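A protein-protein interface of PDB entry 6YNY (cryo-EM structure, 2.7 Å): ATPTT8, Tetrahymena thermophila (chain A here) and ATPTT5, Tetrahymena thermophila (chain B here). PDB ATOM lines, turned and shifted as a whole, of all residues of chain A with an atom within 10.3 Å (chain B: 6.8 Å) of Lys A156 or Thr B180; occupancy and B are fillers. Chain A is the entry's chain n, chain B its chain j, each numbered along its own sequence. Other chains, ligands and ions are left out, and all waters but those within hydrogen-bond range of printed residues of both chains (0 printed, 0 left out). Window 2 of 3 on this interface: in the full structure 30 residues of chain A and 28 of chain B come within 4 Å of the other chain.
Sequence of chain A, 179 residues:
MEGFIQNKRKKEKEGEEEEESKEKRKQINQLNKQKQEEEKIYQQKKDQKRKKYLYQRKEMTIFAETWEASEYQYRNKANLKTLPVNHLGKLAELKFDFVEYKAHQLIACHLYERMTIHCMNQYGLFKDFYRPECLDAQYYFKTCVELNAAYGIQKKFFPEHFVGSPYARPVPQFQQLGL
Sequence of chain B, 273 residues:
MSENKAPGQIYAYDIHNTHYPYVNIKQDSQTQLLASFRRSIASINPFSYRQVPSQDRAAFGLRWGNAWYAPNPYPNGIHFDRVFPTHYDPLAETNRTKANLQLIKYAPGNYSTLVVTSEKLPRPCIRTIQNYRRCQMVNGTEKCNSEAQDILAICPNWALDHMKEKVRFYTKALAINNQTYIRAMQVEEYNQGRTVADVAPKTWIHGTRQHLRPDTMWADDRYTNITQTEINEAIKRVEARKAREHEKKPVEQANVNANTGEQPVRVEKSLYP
The side-chain amino group (NZ) of Lys B172 lies within salt-bridge range of the side-chain carboxylate (OE2) of Glu A160. The side-chain amino group (NZ) of Lys B172 lies within hydrogen-bond range of the backbone carbonyl oxygen (O) of Phe A157. The side-chain hydroxyl of Thr B180 lies within hydrogen-bond range of the side-chain amino group of Lys A156, 3.2 Å away.
The side-chain hydroxyl (OG1) of Thr B180 is in hydrogen-bond range of the guanidinium group (NH2) of Arg B183. The backbone carbonyl oxygen (O) of Ile B176 sits at hydrogen-bond distance from the side-chain hydroxyl (OG1) of Thr B180, at 2.8 Å.
Lys A156 touches Ile B176. Phe A157 touches Ile B176 (CA to CD1, 3.9 Å). Phe A157 touches Asn B177. CD1 of Phe A158 touches NZ of Lys B172, 3.8 Å away.
Lys A156 touches just these residues of chain B: Ile B176 and Thr B180. Of chain A, only Lys A156 comes within 4 Å of Thr B180. Ile B176 touches two residues of chain A. Of chain A, only Phe A157 comes within 4 Å of Asn B177. No residue of chain A comes within 4 Å of Arg B183. Of the printed residues of chain A, Lys B172 touches Phe A157 (2.8 Å), Phe A158 (3.8 Å) and Glu A160 (2.5 Å). Printed residues of chain B within 4 Å of Phe A157: Lys B172, Ile B176 and Asn B177. Printed residues of chain B within 4 Å of Phe A158: Lys B172. The nearest residue of chain B that does not touch Lys A156 is Asn B177 (4.2 Å).
Printed residues of chain B that touch a printed residue of chain A: Lys B172, Ile B176, Asn B177 and Thr B180. Hydrophobic or aromatic side chains of chain B that line the printed part of chain A: Ile B176. Of the 22 printed residues of chain A, 4 touch a printed residue of chain B. Among the printed residues, Asp or Glu carboxylates within 4 Å of a Lys or Arg side-chain nitrogen of the other chain: Glu A160 with Lys B172 (2.5 Å).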
ATOM      1  N   THR A  61     -18.805  -4.910  10.292  1.00  0.00           N
ATOM      2  CA  THR A  61     -17.498  -4.509  10.794  1.00  0.00           C
ATOM      3  C   THR A  61     -16.534  -4.264   9.644  1.00  0.00           C
ATOM      4  O   THR A  61     -16.584  -4.948   8.623  1.00  0.00           O
ATOM      5  CB  THR A  61     -16.904  -5.573  11.733  1.00  0.00           C
ATOM      6  OG1 THR A  61     -17.790  -5.794  12.834  1.00  0.00           O
ATOM      7  CG2 THR A  61     -15.558  -5.130  12.264  1.00  0.00           C
ATOM      8  N   ILE A  62     -15.659  -3.280   9.813  1.00  0.00           N
ATOM      9  CA  ILE A  62     -14.634  -2.969   8.825  1.00  0.00           C
ATOM     10  C   ILE A  62     -13.377  -3.743   9.195  1.00  0.00           C
ATOM     11  O   ILE A  62     -12.865  -3.617  10.313  1.00  0.00           O
ATOM     12  CB  ILE A  62     -14.356  -1.463   8.763  1.00  0.00           C
ATOM     13  CG1 ILE A  62     -15.648  -0.698   8.491  1.00  0.00           C
ATOM     14  CG2 ILE A  62     -13.347  -1.158   7.678  1.00  0.00           C
ATOM     15  CD1 ILE A  62     -15.485   0.794   8.514  1.00  0.00           C
ATOM     16  N   PHE A  63     -12.881  -4.541   8.258  1.00  0.00           N
ATOM     17  CA  PHE A  63     -11.700  -5.370   8.455  1.00  0.00           C
ATOM     18  C   PHE A  63     -10.488  -4.796   7.730  1.00  0.00           C
ATOM     19  O   PHE A  63      -9.685  -5.527   7.151  1.00  0.00           O
ATOM     20  CB  PHE A  63     -11.973  -6.800   8.010  1.00  0.00           C
ATOM     21  CG  PHE A  63     -13.053  -7.475   8.800  1.00  0.00           C
ATOM     22  CD1 PHE A  63     -12.819  -7.889  10.096  1.00  0.00           C
ATOM     23  CD2 PHE A  63     -14.302  -7.692   8.254  1.00  0.00           C
ATOM     24  CE1 PHE A  63     -13.804  -8.505  10.828  1.00  0.00           C
ATOM     25  CE2 PHE A  63     -15.291  -8.311   8.988  1.00  0.00           C
ATOM     26  CZ  PHE A  63     -15.040  -8.715  10.274  1.00  0.00           C
ATOM     27  N   GLU A  71     -19.252   3.865  -0.263  1.00  0.00           N
ATOM     28  CA  GLU A  71     -19.912   2.659   0.219  1.00  0.00           C
ATOM     29  C   GLU A  71     -20.727   2.892   1.481  1.00  0.00           C
ATOM     30  O   GLU A  71     -21.517   2.020   1.852  1.00  0.00           O
ATOM     31  CB  GLU A  71     -18.881   1.563   0.471  1.00  0.00           C
ATOM     32  CG  GLU A  71     -18.288   0.989  -0.797  1.00  0.00           C
ATOM     33  CD  GLU A  71     -17.268  -0.097  -0.529  1.00  0.00           C
ATOM     34  OE1 GLU A  71     -16.918  -0.310   0.652  1.00  0.00           O
ATOM     35  OE2 GLU A  71     -16.816  -0.740  -1.499  1.00  0.00           O
ATOM     36  N   TYR A  72     -20.559   4.035   2.142  1.00  0.00           N
ATOM     37  CA  TYR A  72     -21.328   4.369   3.334  1.00  0.00           C
ATOM     38  C   TYR A  72     -22.203   5.596   3.115  1.00  0.00           C
ATOM     39  O   TYR A  72     -22.620   6.241   4.080  1.00  0.00           O
ATOM     40  CB  TYR A  72     -20.393   4.562   4.527  1.00  0.00           C
ATOM     41  CG  TYR A  72     -19.725   3.276   4.942  1.00  0.00           C
ATOM     42  CD1 TYR A  72     -18.519   2.886   4.385  1.00  0.00           C
ATOM     43  CD2 TYR A  72     -20.313   2.439   5.873  1.00  0.00           C
ATOM     44  CE1 TYR A  72     -17.916   1.708   4.754  1.00  0.00           C
ATOM     45  CE2 TYR A  72     -19.716   1.260   6.247  1.00  0.00           C
ATOM     46  CZ  TYR A  72     -18.519   0.899   5.684  1.00  0.00           C
ATOM     47  OH  TYR A  72     -17.924  -0.280   6.057  1.00  0.00           O
ATOM     48  N   ASN A 148     -20.206   4.573  14.053  1.00  0.00           N
ATOM     49  CA  ASN A 148     -19.736   3.359  13.401  1.00  0.00           C
ATOM     50  C   ASN A 148     -20.551   2.144  13.817  1.00  0.00           C
ATOM     51  O   ASN A 148     -20.753   1.229  13.014  1.00  0.00           O
ATOM     52  CB  ASN A 148     -18.256   3.150  13.702  1.00  0.00           C
ATOM     53  CG  ASN A 148     -17.360   3.883  12.733  1.00  0.00           C
ATOM     54  OD1 ASN A 148     -17.004   3.359  11.680  1.00  0.00           O
ATOM     55  ND2 ASN A 148     -16.997   5.106  13.078  1.00  0.00           N
ATOM     56  N   ALA A 149     -21.026   2.116  15.061  1.00  0.00           N
ATOM     57  CA  ALA A 149     -21.917   1.040  15.477  1.00  0.00           C
ATOM     58  C   ALA A 149     -23.248   1.118  14.746  1.00  0.00           C
ATOM     59  O   ALA A 149     -23.837   0.088  14.401  1.00  0.00           O
ATOM     60  CB  ALA A 149     -22.137   1.092  16.985  1.00  0.00           C
ATOM     61  N   ALA A 150     -23.738   2.332  14.497  1.00  0.00           N
ATOM     62  CA  ALA A 150     -24.999   2.488  13.784  1.00  0.00           C
ATOM     63  C   ALA A 150     -24.836   2.206  12.298  1.00  0.00           C
ATOM     64  O   ALA A 150     -25.676   1.530  11.696  1.00  0.00           O
ATOM     65  CB  ALA A 150     -25.549   3.891  14.009  1.00  0.00           C
ATOM     66  N   TYR A 151     -23.770   2.720  11.687  1.00  0.00           N
ATOM     67  CA  TYR A 151     -23.517   2.414  10.286  1.00  0.00           C
ATOM     68  C   TYR A 151     -23.216   0.937  10.083  1.00  0.00           C
ATOM     69  O   TYR A 151     -23.591   0.366   9.054  1.00  0.00           O
ATOM     70  CB  TYR A 151     -22.362   3.261   9.761  1.00  0.00           C
ATOM     71  CG  TYR A 151     -22.764   4.636   9.294  1.00  0.00           C
ATOM     72  CD1 TYR A 151     -23.399   4.812   8.077  1.00  0.00           C
ATOM     73  CD2 TYR A 151     -22.495   5.758  10.057  1.00  0.00           C
ATOM     74  CE1 TYR A 151     -23.762   6.058   7.640  1.00  0.00           C
ATOM     75  CE2 TYR A 151     -22.855   7.013   9.626  1.00  0.00           C
ATOM     76  CZ  TYR A 151     -23.488   7.158   8.416  1.00  0.00           C
ATOM     77  OH  TYR A 151     -23.850   8.408   7.980  1.00  0.00           O
ATOM     78  N   GLY A 152     -22.541   0.307  11.042  1.00  0.00           N
ATOM     79  CA  GLY A 152     -22.254  -1.110  10.921  1.00  0.00           C
ATOM     80  C   GLY A 152     -23.507  -1.961  10.971  1.00  0.00           C
ATOM     81  O   GLY A 152     -23.646  -2.923  10.213  1.00  0.00           O
ATOM     82  N   ILE A 153     -24.434  -1.621  11.864  1.00  0.00           N
ATOM     83  CA  ILE A 153     -25.697  -2.343  11.931  1.00  0.00           C
ATOM     84  C   ILE A 153     -26.530  -2.067  10.690  1.00  0.00           C
ATOM     85  O   ILE A 153     -27.157  -2.974  10.130  1.00  0.00           O
ATOM     86  CB  ILE A 153     -26.453  -1.966  13.214  1.00  0.00           C
ATOM     87  CG1 ILE A 153     -25.696  -2.468  14.441  1.00  0.00           C
ATOM     88  CG2 ILE A 153     -27.839  -2.541  13.182  1.00  0.00           C
ATOM     89  CD1 ILE A 153     -26.097  -1.799  15.729  1.00  0.00           C
ATOM     90  N   GLN A 154     -26.558  -0.813  10.242  1.00  0.00           N
ATOM     91  CA  GLN A 154     -27.276  -0.483   9.020  1.00  0.00           C
ATOM     92  C   GLN A 154     -26.652  -1.165   7.811  1.00  0.00           C
ATOM     93  O   GLN A 154     -27.346  -1.461   6.835  1.00  0.00           O
ATOM     94  CB  GLN A 154     -27.298   1.033   8.838  1.00  0.00           C
ATOM     95  CG  GLN A 154     -28.235   1.528   7.769  1.00  0.00           C
ATOM     96  CD  GLN A 154     -28.314   3.032   7.729  1.00  0.00           C
ATOM     97  OE1 GLN A 154     -27.519   3.725   8.360  1.00  0.00           O
ATOM     98  NE2 GLN A 154     -29.284   3.548   6.994  1.00  0.00           N
ATOM     99  N   LYS A 155     -25.344  -1.419   7.857  1.00  0.00           N
ATOM    100  CA  LYS A 155     -24.685  -2.154   6.785  1.00  0.00           C
ATOM    101  C   LYS A 155     -25.020  -3.635   6.831  1.00  0.00           C
ATOM    102  O   LYS A 155     -24.990  -4.311   5.797  1.00  0.00           O
ATOM    103  CB  LYS A 155     -23.174  -1.968   6.880  1.00  0.00           C
ATOM    104  CG  LYS A 155     -22.632  -0.882   6.006  1.00  0.00           C
ATOM    105  CD  LYS A 155     -22.537  -1.343   4.577  1.00  0.00           C
ATOM    106  CE  LYS A 155     -21.980  -0.258   3.696  1.00  0.00           C
ATOM    107  NZ  LYS A 155     -21.880  -0.692   2.293  1.00  0.00           N
ATOM    108  N   LYS A 156     -25.331  -4.153   8.016  1.00  0.00           N
ATOM    109  CA  LYS A 156     -25.605  -5.574   8.175  1.00  0.00           C
ATOM    110  C   LYS A 156     -27.037  -5.917   7.793  1.00  0.00           C
ATOM    111  O   LYS A 156     -27.275  -6.912   7.101  1.00  0.00           O
ATOM    112  CB  LYS A 156     -25.332  -5.983   9.618  1.00  0.00           C
ATOM    113  CG  LYS A 156     -25.462  -7.457   9.908  1.00  0.00           C
ATOM    114  CD  LYS A 156     -25.109  -7.735  11.352  1.00  0.00           C
ATOM    115  CE  LYS A 156     -25.261  -9.194  11.711  1.00  0.00           C
ATOM    116  NZ  LYS A 156     -24.321 -10.058  10.971  1.00  0.00           N
ATOM    117  N   PHE A 157     -27.996  -5.097   8.218  1.00  0.00           N
ATOM    118  CA  PHE A 157     -29.405  -5.376   8.007  1.00  0.00           C
ATOM    119  C   PHE A 157     -30.059  -4.512   6.943  1.00  0.00           C
ATOM    120  O   PHE A 157     -31.152  -4.857   6.486  1.00  0.00           O
ATOM    121  CB  PHE A 157     -30.169  -5.202   9.322  1.00  0.00           C
ATOM    122  CG  PHE A 157     -29.731  -6.142  10.400  1.00  0.00           C
ATOM    123  CD1 PHE A 157     -30.248  -7.417  10.475  1.00  0.00           C
ATOM    124  CD2 PHE A 157     -28.799  -5.750  11.339  1.00  0.00           C
ATOM    125  CE1 PHE A 157     -29.846  -8.278  11.464  1.00  0.00           C
ATOM    126  CE2 PHE A 157     -28.397  -6.610  12.327  1.00  0.00           C
ATOM    127  CZ  PHE A 157     -28.921  -7.874  12.389  1.00  0.00           C
ATOM    128  N   PHE A 158     -29.431  -3.412   6.541  1.00  0.00           N
ATOM    129  CA  PHE A 158     -29.956  -2.541   5.489  1.00  0.00           C
ATOM    130  C   PHE A 158     -28.867  -2.253   4.464  1.00  0.00           C
ATOM    131  O   PHE A 158     -28.548  -1.096   4.184  1.00  0.00           O
ATOM    132  CB  PHE A 158     -30.492  -1.240   6.075  1.00  0.00           C
ATOM    133  CG  PHE A 158     -31.483  -1.424   7.180  1.00  0.00           C
ATOM    134  CD1 PHE A 158     -32.837  -1.369   6.926  1.00  0.00           C
ATOM    135  CD2 PHE A 158     -31.062  -1.629   8.476  1.00  0.00           C
ATOM    136  CE1 PHE A 158     -33.747  -1.522   7.943  1.00  0.00           C
ATOM    137  CE2 PHE A 158     -31.971  -1.786   9.493  1.00  0.00           C
ATOM    138  CZ  PHE A 158     -33.312  -1.730   9.225  1.00  0.00           C
ATOM    139  N   PRO A 159     -28.274  -3.293   3.877  1.00  0.00           N
ATOM    140  CA  PRO A 159     -27.253  -3.060   2.848  1.00  0.00           C
ATOM    141  C   PRO A 159     -27.810  -2.430   1.591  1.00  0.00           C
ATOM    142  O   PRO A 159     -27.052  -1.807   0.838  1.00  0.00           O
ATOM    143  CB  PRO A 159     -26.706  -4.464   2.577  1.00  0.00           C
ATOM    144  CG  PRO A 159     -27.811  -5.368   2.954  1.00  0.00           C
ATOM    145  CD  PRO A 159     -28.519  -4.727   4.088  1.00  0.00           C
ATOM    146  N   GLU A 160     -29.111  -2.569   1.348  1.00  0.00           N
ATOM    147  CA  GLU A 160     -29.762  -1.977   0.188  1.00  0.00           C
ATOM    148  C   GLU A 160     -29.883  -0.463   0.284  1.00  0.00           C
ATOM    149  O   GLU A 160     -30.299   0.169  -0.693  1.00  0.00           O
ATOM    150  CB  GLU A 160     -31.146  -2.597   0.004  1.00  0.00           C
ATOM    151  CG  GLU A 160     -32.073  -2.475   1.213  1.00  0.00           C
ATOM    152  CD  GLU A 160     -31.900  -3.599   2.211  1.00  0.00           C
ATOM    153  OE1 GLU A 160     -30.954  -4.397   2.051  1.00  0.00           O
ATOM    154  OE2 GLU A 160     -32.707  -3.684   3.158  1.00  0.00           O
ATOM    155  N   HIS A 161     -29.539   0.132   1.425  1.00  0.00           N
ATOM    156  CA  HIS A 161     -29.631   1.574   1.585  1.00  0.00           C
ATOM    157  C   HIS A 161     -28.439   2.313   1.000  1.00  0.00           C
ATOM    158  O   HIS A 161     -28.555   3.503   0.695  1.00  0.00           O
ATOM    159  CB  HIS A 161     -29.745   1.933   3.067  1.00  0.00           C
ATOM    160  CG  HIS A 161     -31.080   1.636   3.667  1.00  0.00           C
ATOM    161  ND1 HIS A 161     -31.375   1.913   4.983  1.00  0.00           N
ATOM    162  CD2 HIS A 161     -32.202   1.097   3.135  1.00  0.00           C
ATOM    163  CE1 HIS A 161     -32.619   1.556   5.237  1.00  0.00           C
ATOM    164  NE2 HIS A 161     -33.143   1.056   4.133  1.00  0.00           N
ATOM    165  N   PHE A 162     -27.309   1.642   0.832  1.00  0.00           N
ATOM    166  CA  PHE A 162     -26.048   2.294   0.522  1.00  0.00           C
ATOM    167  C   PHE A 162     -25.705   2.201  -0.959  1.00  0.00           C
ATOM    168  O   PHE A 162     -26.159   1.312  -1.682  1.00  0.00           O
ATOM    169  CB  PHE A 162     -24.919   1.680   1.347  1.00  0.00           C
ATOM    170  CG  PHE A 162     -25.109   1.821   2.819  1.00  0.00           C
ATOM    171  CD1 PHE A 162     -24.667   2.945   3.482  1.00  0.00           C
ATOM    172  CD2 PHE A 162     -25.734   0.831   3.542  1.00  0.00           C
ATOM    173  CE1 PHE A 162     -24.844   3.075   4.834  1.00  0.00           C
ATOM    174  CE2 PHE A 162     -25.914   0.957   4.892  1.00  0.00           C
ATOM    175  CZ  PHE A 162     -25.469   2.079   5.541  1.00  0.00           C
ATOM    176  N   SER A 165     -24.278  -1.165  -3.409  1.00  0.00           N
ATOM    177  CA  SER A 165     -24.981  -2.423  -3.229  1.00  0.00           C
ATOM    178  C   SER A 165     -25.810  -2.738  -4.471  1.00  0.00           C
ATOM    179  O   SER A 165     -26.436  -1.842  -5.041  1.00  0.00           O
ATOM    180  CB  SER A 165     -25.890  -2.363  -2.008  1.00  0.00           C
ATOM    181  OG  SER A 165     -26.543  -3.600  -1.798  1.00  0.00           O
ATOM    182  N   TYR A 167     -28.540  -4.300  -4.550  1.00  0.00           N
ATOM    183  CA  TYR A 167     -29.947  -4.299  -4.190  1.00  0.00           C
ATOM    184  C   TYR A 167     -30.511  -2.898  -4.007  1.00  0.00           C
ATOM    185  O   TYR A 167     -31.730  -2.752  -3.881  1.00  0.00           O
ATOM    186  CB  TYR A 167     -30.157  -5.106  -2.905  1.00  0.00           C
ATOM    187  CG  TYR A 167     -29.461  -6.440  -2.917  1.00  0.00           C
ATOM    188  CD1 TYR A 167     -29.957  -7.498  -3.661  1.00  0.00           C
ATOM    189  CD2 TYR A 167     -28.305  -6.644  -2.185  1.00  0.00           C
ATOM    190  CE1 TYR A 167     -29.320  -8.715  -3.677  1.00  0.00           C
ATOM    191  CE2 TYR A 167     -27.662  -7.858  -2.196  1.00  0.00           C
ATOM    192  CZ  TYR A 167     -28.174  -8.890  -2.944  1.00  0.00           C
ATOM    193  OH  TYR A 167     -27.539 -10.107  -2.959  1.00  0.00           O
ATOM    194  N   LYS B 172     -36.140 -10.576   6.868  1.00  0.00           N
ATOM    195  CA  LYS B 172     -34.817 -10.295   6.325  1.00  0.00           C
ATOM    196  C   LYS B 172     -33.745 -10.429   7.396  1.00  0.00           C
ATOM    197  O   LYS B 172     -32.712 -11.070   7.180  1.00  0.00           O
ATOM    198  CB  LYS B 172     -34.801  -8.894   5.722  1.00  0.00           C
ATOM    199  CG  LYS B 172     -33.524  -8.524   5.002  1.00  0.00           C
ATOM    200  CD  LYS B 172     -33.091  -7.111   5.329  1.00  0.00           C
ATOM    201  CE  LYS B 172     -34.127  -6.091   4.924  1.00  0.00           C
ATOM    202  NZ  LYS B 172     -33.692  -4.706   5.221  1.00  0.00           N
ATOM    203  N   ALA B 175     -32.937 -14.108   8.246  1.00  0.00           N
ATOM    204  CA  ALA B 175     -32.032 -14.798   7.337  1.00  0.00           C
ATOM    205  C   ALA B 175     -30.605 -14.295   7.488  1.00  0.00           C
ATOM    206  O   ALA B 175     -29.652 -15.070   7.361  1.00  0.00           O
ATOM    207  CB  ALA B 175     -32.508 -14.622   5.901  1.00  0.00           C
ATOM    208  N   ILE B 176     -30.434 -13.000   7.751  1.00  0.00           N
ATOM    209  CA  ILE B 176     -29.093 -12.452   7.914  1.00  0.00           C
ATOM    210  C   ILE B 176     -28.439 -13.005   9.171  1.00  0.00           C
ATOM    211  O   ILE B 176     -27.230 -13.264   9.195  1.00  0.00           O
ATOM    212  CB  ILE B 176     -29.154 -10.917   7.922  1.00  0.00           C
ATOM    213  CG1 ILE B 176     -29.428 -10.410   6.508  1.00  0.00           C
ATOM    214  CG2 ILE B 176     -27.869 -10.328   8.468  1.00  0.00           C
ATOM    215  CD1 ILE B 176     -29.784  -8.961   6.425  1.00  0.00           C
ATOM    216  N   ASN B 177     -29.220 -13.199  10.232  1.00  0.00           N
ATOM    217  CA  ASN B 177     -28.669 -13.775  11.449  1.00  0.00           C
ATOM    218  C   ASN B 177     -28.397 -15.265  11.296  1.00  0.00           C
ATOM    219  O   ASN B 177     -27.498 -15.799  11.955  1.00  0.00           O
ATOM    220  CB  ASN B 177     -29.613 -13.523  12.620  1.00  0.00           C
ATOM    221  CG  ASN B 177     -29.578 -12.089  13.097  1.00  0.00           C
ATOM    222  OD1 ASN B 177     -28.553 -11.418  13.006  1.00  0.00           O
ATOM    223  ND2 ASN B 177     -30.699 -11.611  13.611  1.00  0.00           N
ATOM    224  N   ASN B 178     -29.155 -15.952  10.441  1.00  0.00           N
ATOM    225  CA  ASN B 178     -28.923 -17.374  10.223  1.00  0.00           C
ATOM    226  C   ASN B 178     -27.778 -17.626   9.251  1.00  0.00           C
ATOM    227  O   ASN B 178     -27.085 -18.641   9.371  1.00  0.00           O
ATOM    228  CB  ASN B 178     -30.201 -18.047   9.726  1.00  0.00           C
ATOM    229  CG  ASN B 178     -31.123 -18.445  10.856  1.00  0.00           C
ATOM    230  OD1 ASN B 178     -31.000 -19.531  11.418  1.00  0.00           O
ATOM    231  ND2 ASN B 178     -32.054 -17.571  11.195  1.00  0.00           N
ATOM    232  N   GLN B 179     -27.564 -16.731   8.288  1.00  0.00           N
ATOM    233  CA  GLN B 179     -26.377 -16.835   7.449  1.00  0.00           C
ATOM    234  C   GLN B 179     -25.113 -16.636   8.272  1.00  0.00           C
ATOM    235  O   GLN B 179     -24.118 -17.342   8.080  1.00  0.00           O
ATOM    236  CB  GLN B 179     -26.435 -15.812   6.318  1.00  0.00           C
ATOM    237  CG  GLN B 179     -27.444 -16.118   5.239  1.00  0.00           C
ATOM    238  CD  GLN B 179     -27.323 -15.178   4.062  1.00  0.00           C
ATOM    239  OE1 GLN B 179     -26.636 -14.161   4.134  1.00  0.00           O
ATOM    240  NE2 GLN B 179     -27.982 -15.516   2.966  1.00  0.00           N
ATOM    241  N   THR B 180     -25.137 -15.672   9.192  1.00  0.00           N
ATOM    242  CA  THR B 180     -24.020 -15.493  10.111  1.00  0.00           C
ATOM    243  C   THR B 180     -23.828 -16.729  10.978  1.00  0.00           C
ATOM    244  O   THR B 180     -22.696 -17.107  11.297  1.00  0.00           O
ATOM    245  CB  THR B 180     -24.264 -14.258  10.977  1.00  0.00           C
ATOM    246  OG1 THR B 180     -24.552 -13.136  10.136  1.00  0.00           O
ATOM    247  CG2 THR B 180     -23.056 -13.938  11.823  1.00  0.00           C
ATOM    248  N   TYR B 181     -24.930 -17.373  11.366  1.00  0.00           N
ATOM    249  CA  TYR B 181     -24.847 -18.613  12.128  1.00  0.00           C
ATOM    250  C   TYR B 181     -24.107 -19.688  11.345  1.00  0.00           C
ATOM    251  O   TYR B 181     -23.277 -20.414  11.902  1.00  0.00           O
ATOM    252  CB  TYR B 181     -26.256 -19.081  12.482  1.00  0.00           C
ATOM    253  CG  TYR B 181     -26.333 -20.296  13.373  1.00  0.00           C
ATOM    254  CD1 TYR B 181     -26.544 -20.164  14.732  1.00  0.00           C
ATOM    255  CD2 TYR B 181     -26.217 -21.574  12.852  1.00  0.00           C
ATOM    256  CE1 TYR B 181     -26.626 -21.263  15.549  1.00  0.00           C
ATOM    257  CE2 TYR B 181     -26.296 -22.681  13.665  1.00  0.00           C
ATOM    258  CZ  TYR B 181     -26.500 -22.519  15.013  1.00  0.00           C
ATOM    259  OH  TYR B 181     -26.584 -23.614  15.836  1.00  0.00           O
ATOM    260  N   ILE B 182     -24.390 -19.797  10.049  1.00  0.00           N
ATOM    261  CA  ILE B 182     -23.773 -20.833   9.231  1.00  0.00           C
ATOM    262  C   ILE B 182     -22.276 -20.591   9.102  1.00  0.00           C
ATOM    263  O   ILE B 182     -21.464 -21.494   9.330  1.00  0.00           O
ATOM    264  CB  ILE B 182     -24.459 -20.893   7.857  1.00  0.00           C
ATOM    265  CG1 ILE B 182     -25.899 -21.366   8.022  1.00  0.00           C
ATOM    266  CG2 ILE B 182     -23.705 -21.809   6.928  1.00  0.00           C
ATOM    267  CD1 ILE B 182     -26.768 -21.083   6.837  1.00  0.00           C
ATOM    268  N   ARG B 183     -21.886 -19.371   8.731  1.00  0.00           N
ATOM    269  CA  ARG B 183     -20.466 -19.067   8.606  1.00  0.00           C
ATOM    270  C   ARG B 183     -19.741 -19.240   9.930  1.00  0.00           C
ATOM    271  O   ARG B 183     -18.544 -19.541   9.950  1.00  0.00           O
ATOM    272  CB  ARG B 183     -20.274 -17.648   8.080  1.00  0.00           C
ATOM    273  CG  ARG B 183     -20.795 -17.430   6.677  1.00  0.00           C
ATOM    274  CD  ARG B 183     -20.354 -16.088   6.140  1.00  0.00           C
ATOM    275  NE  ARG B 183     -20.750 -14.997   7.024  1.00  0.00           N
ATOM    276  CZ  ARG B 183     -21.880 -14.309   6.912  1.00  0.00           C
ATOM    277  NH1 ARG B 183     -22.748 -14.581   5.948  1.00  0.00           N
ATOM    278  NH2 ARG B 183     -22.141 -13.341   7.774  1.00  0.00           N
ATOM    279  N   ALA B 184     -20.446 -19.052  11.044  1.00  0.00           N
ATOM    280  CA  ALA B 184     -19.825 -19.185  12.353  1.00  0.00           C
ATOM    281  C   ALA B 184     -19.638 -20.645  12.738  1.00  0.00           C
ATOM    282  O   ALA B 184     -18.580 -21.023  13.252  1.00  0.00           O
ATOM    283  CB  ALA B 184     -20.668 -18.468  13.398  1.00  0.00           C
ATOM    284  N   MET B 185     -20.649 -21.472  12.502  1.00  0.00           N
ATOM    285  CA  MET B 185     -20.600 -22.882  12.853  1.00  0.00           C
ATOM    286  C   MET B 185     -19.922 -23.729  11.788  1.00  0.00           C
ATOM    287  O   MET B 185     -19.916 -24.957  11.901  1.00  0.00           O
ATOM    288  CB  MET B 185     -22.015 -23.397  13.101  1.00  0.00           C
ATOM    289  CG  MET B 185     -22.771 -22.590  14.127  1.00  0.00           C
ATOM    290  SD  MET B 185     -22.017 -22.609  15.756  1.00  0.00           S
ATOM    291  CE  MET B 185     -22.264 -24.319  16.191  1.00  0.00           C
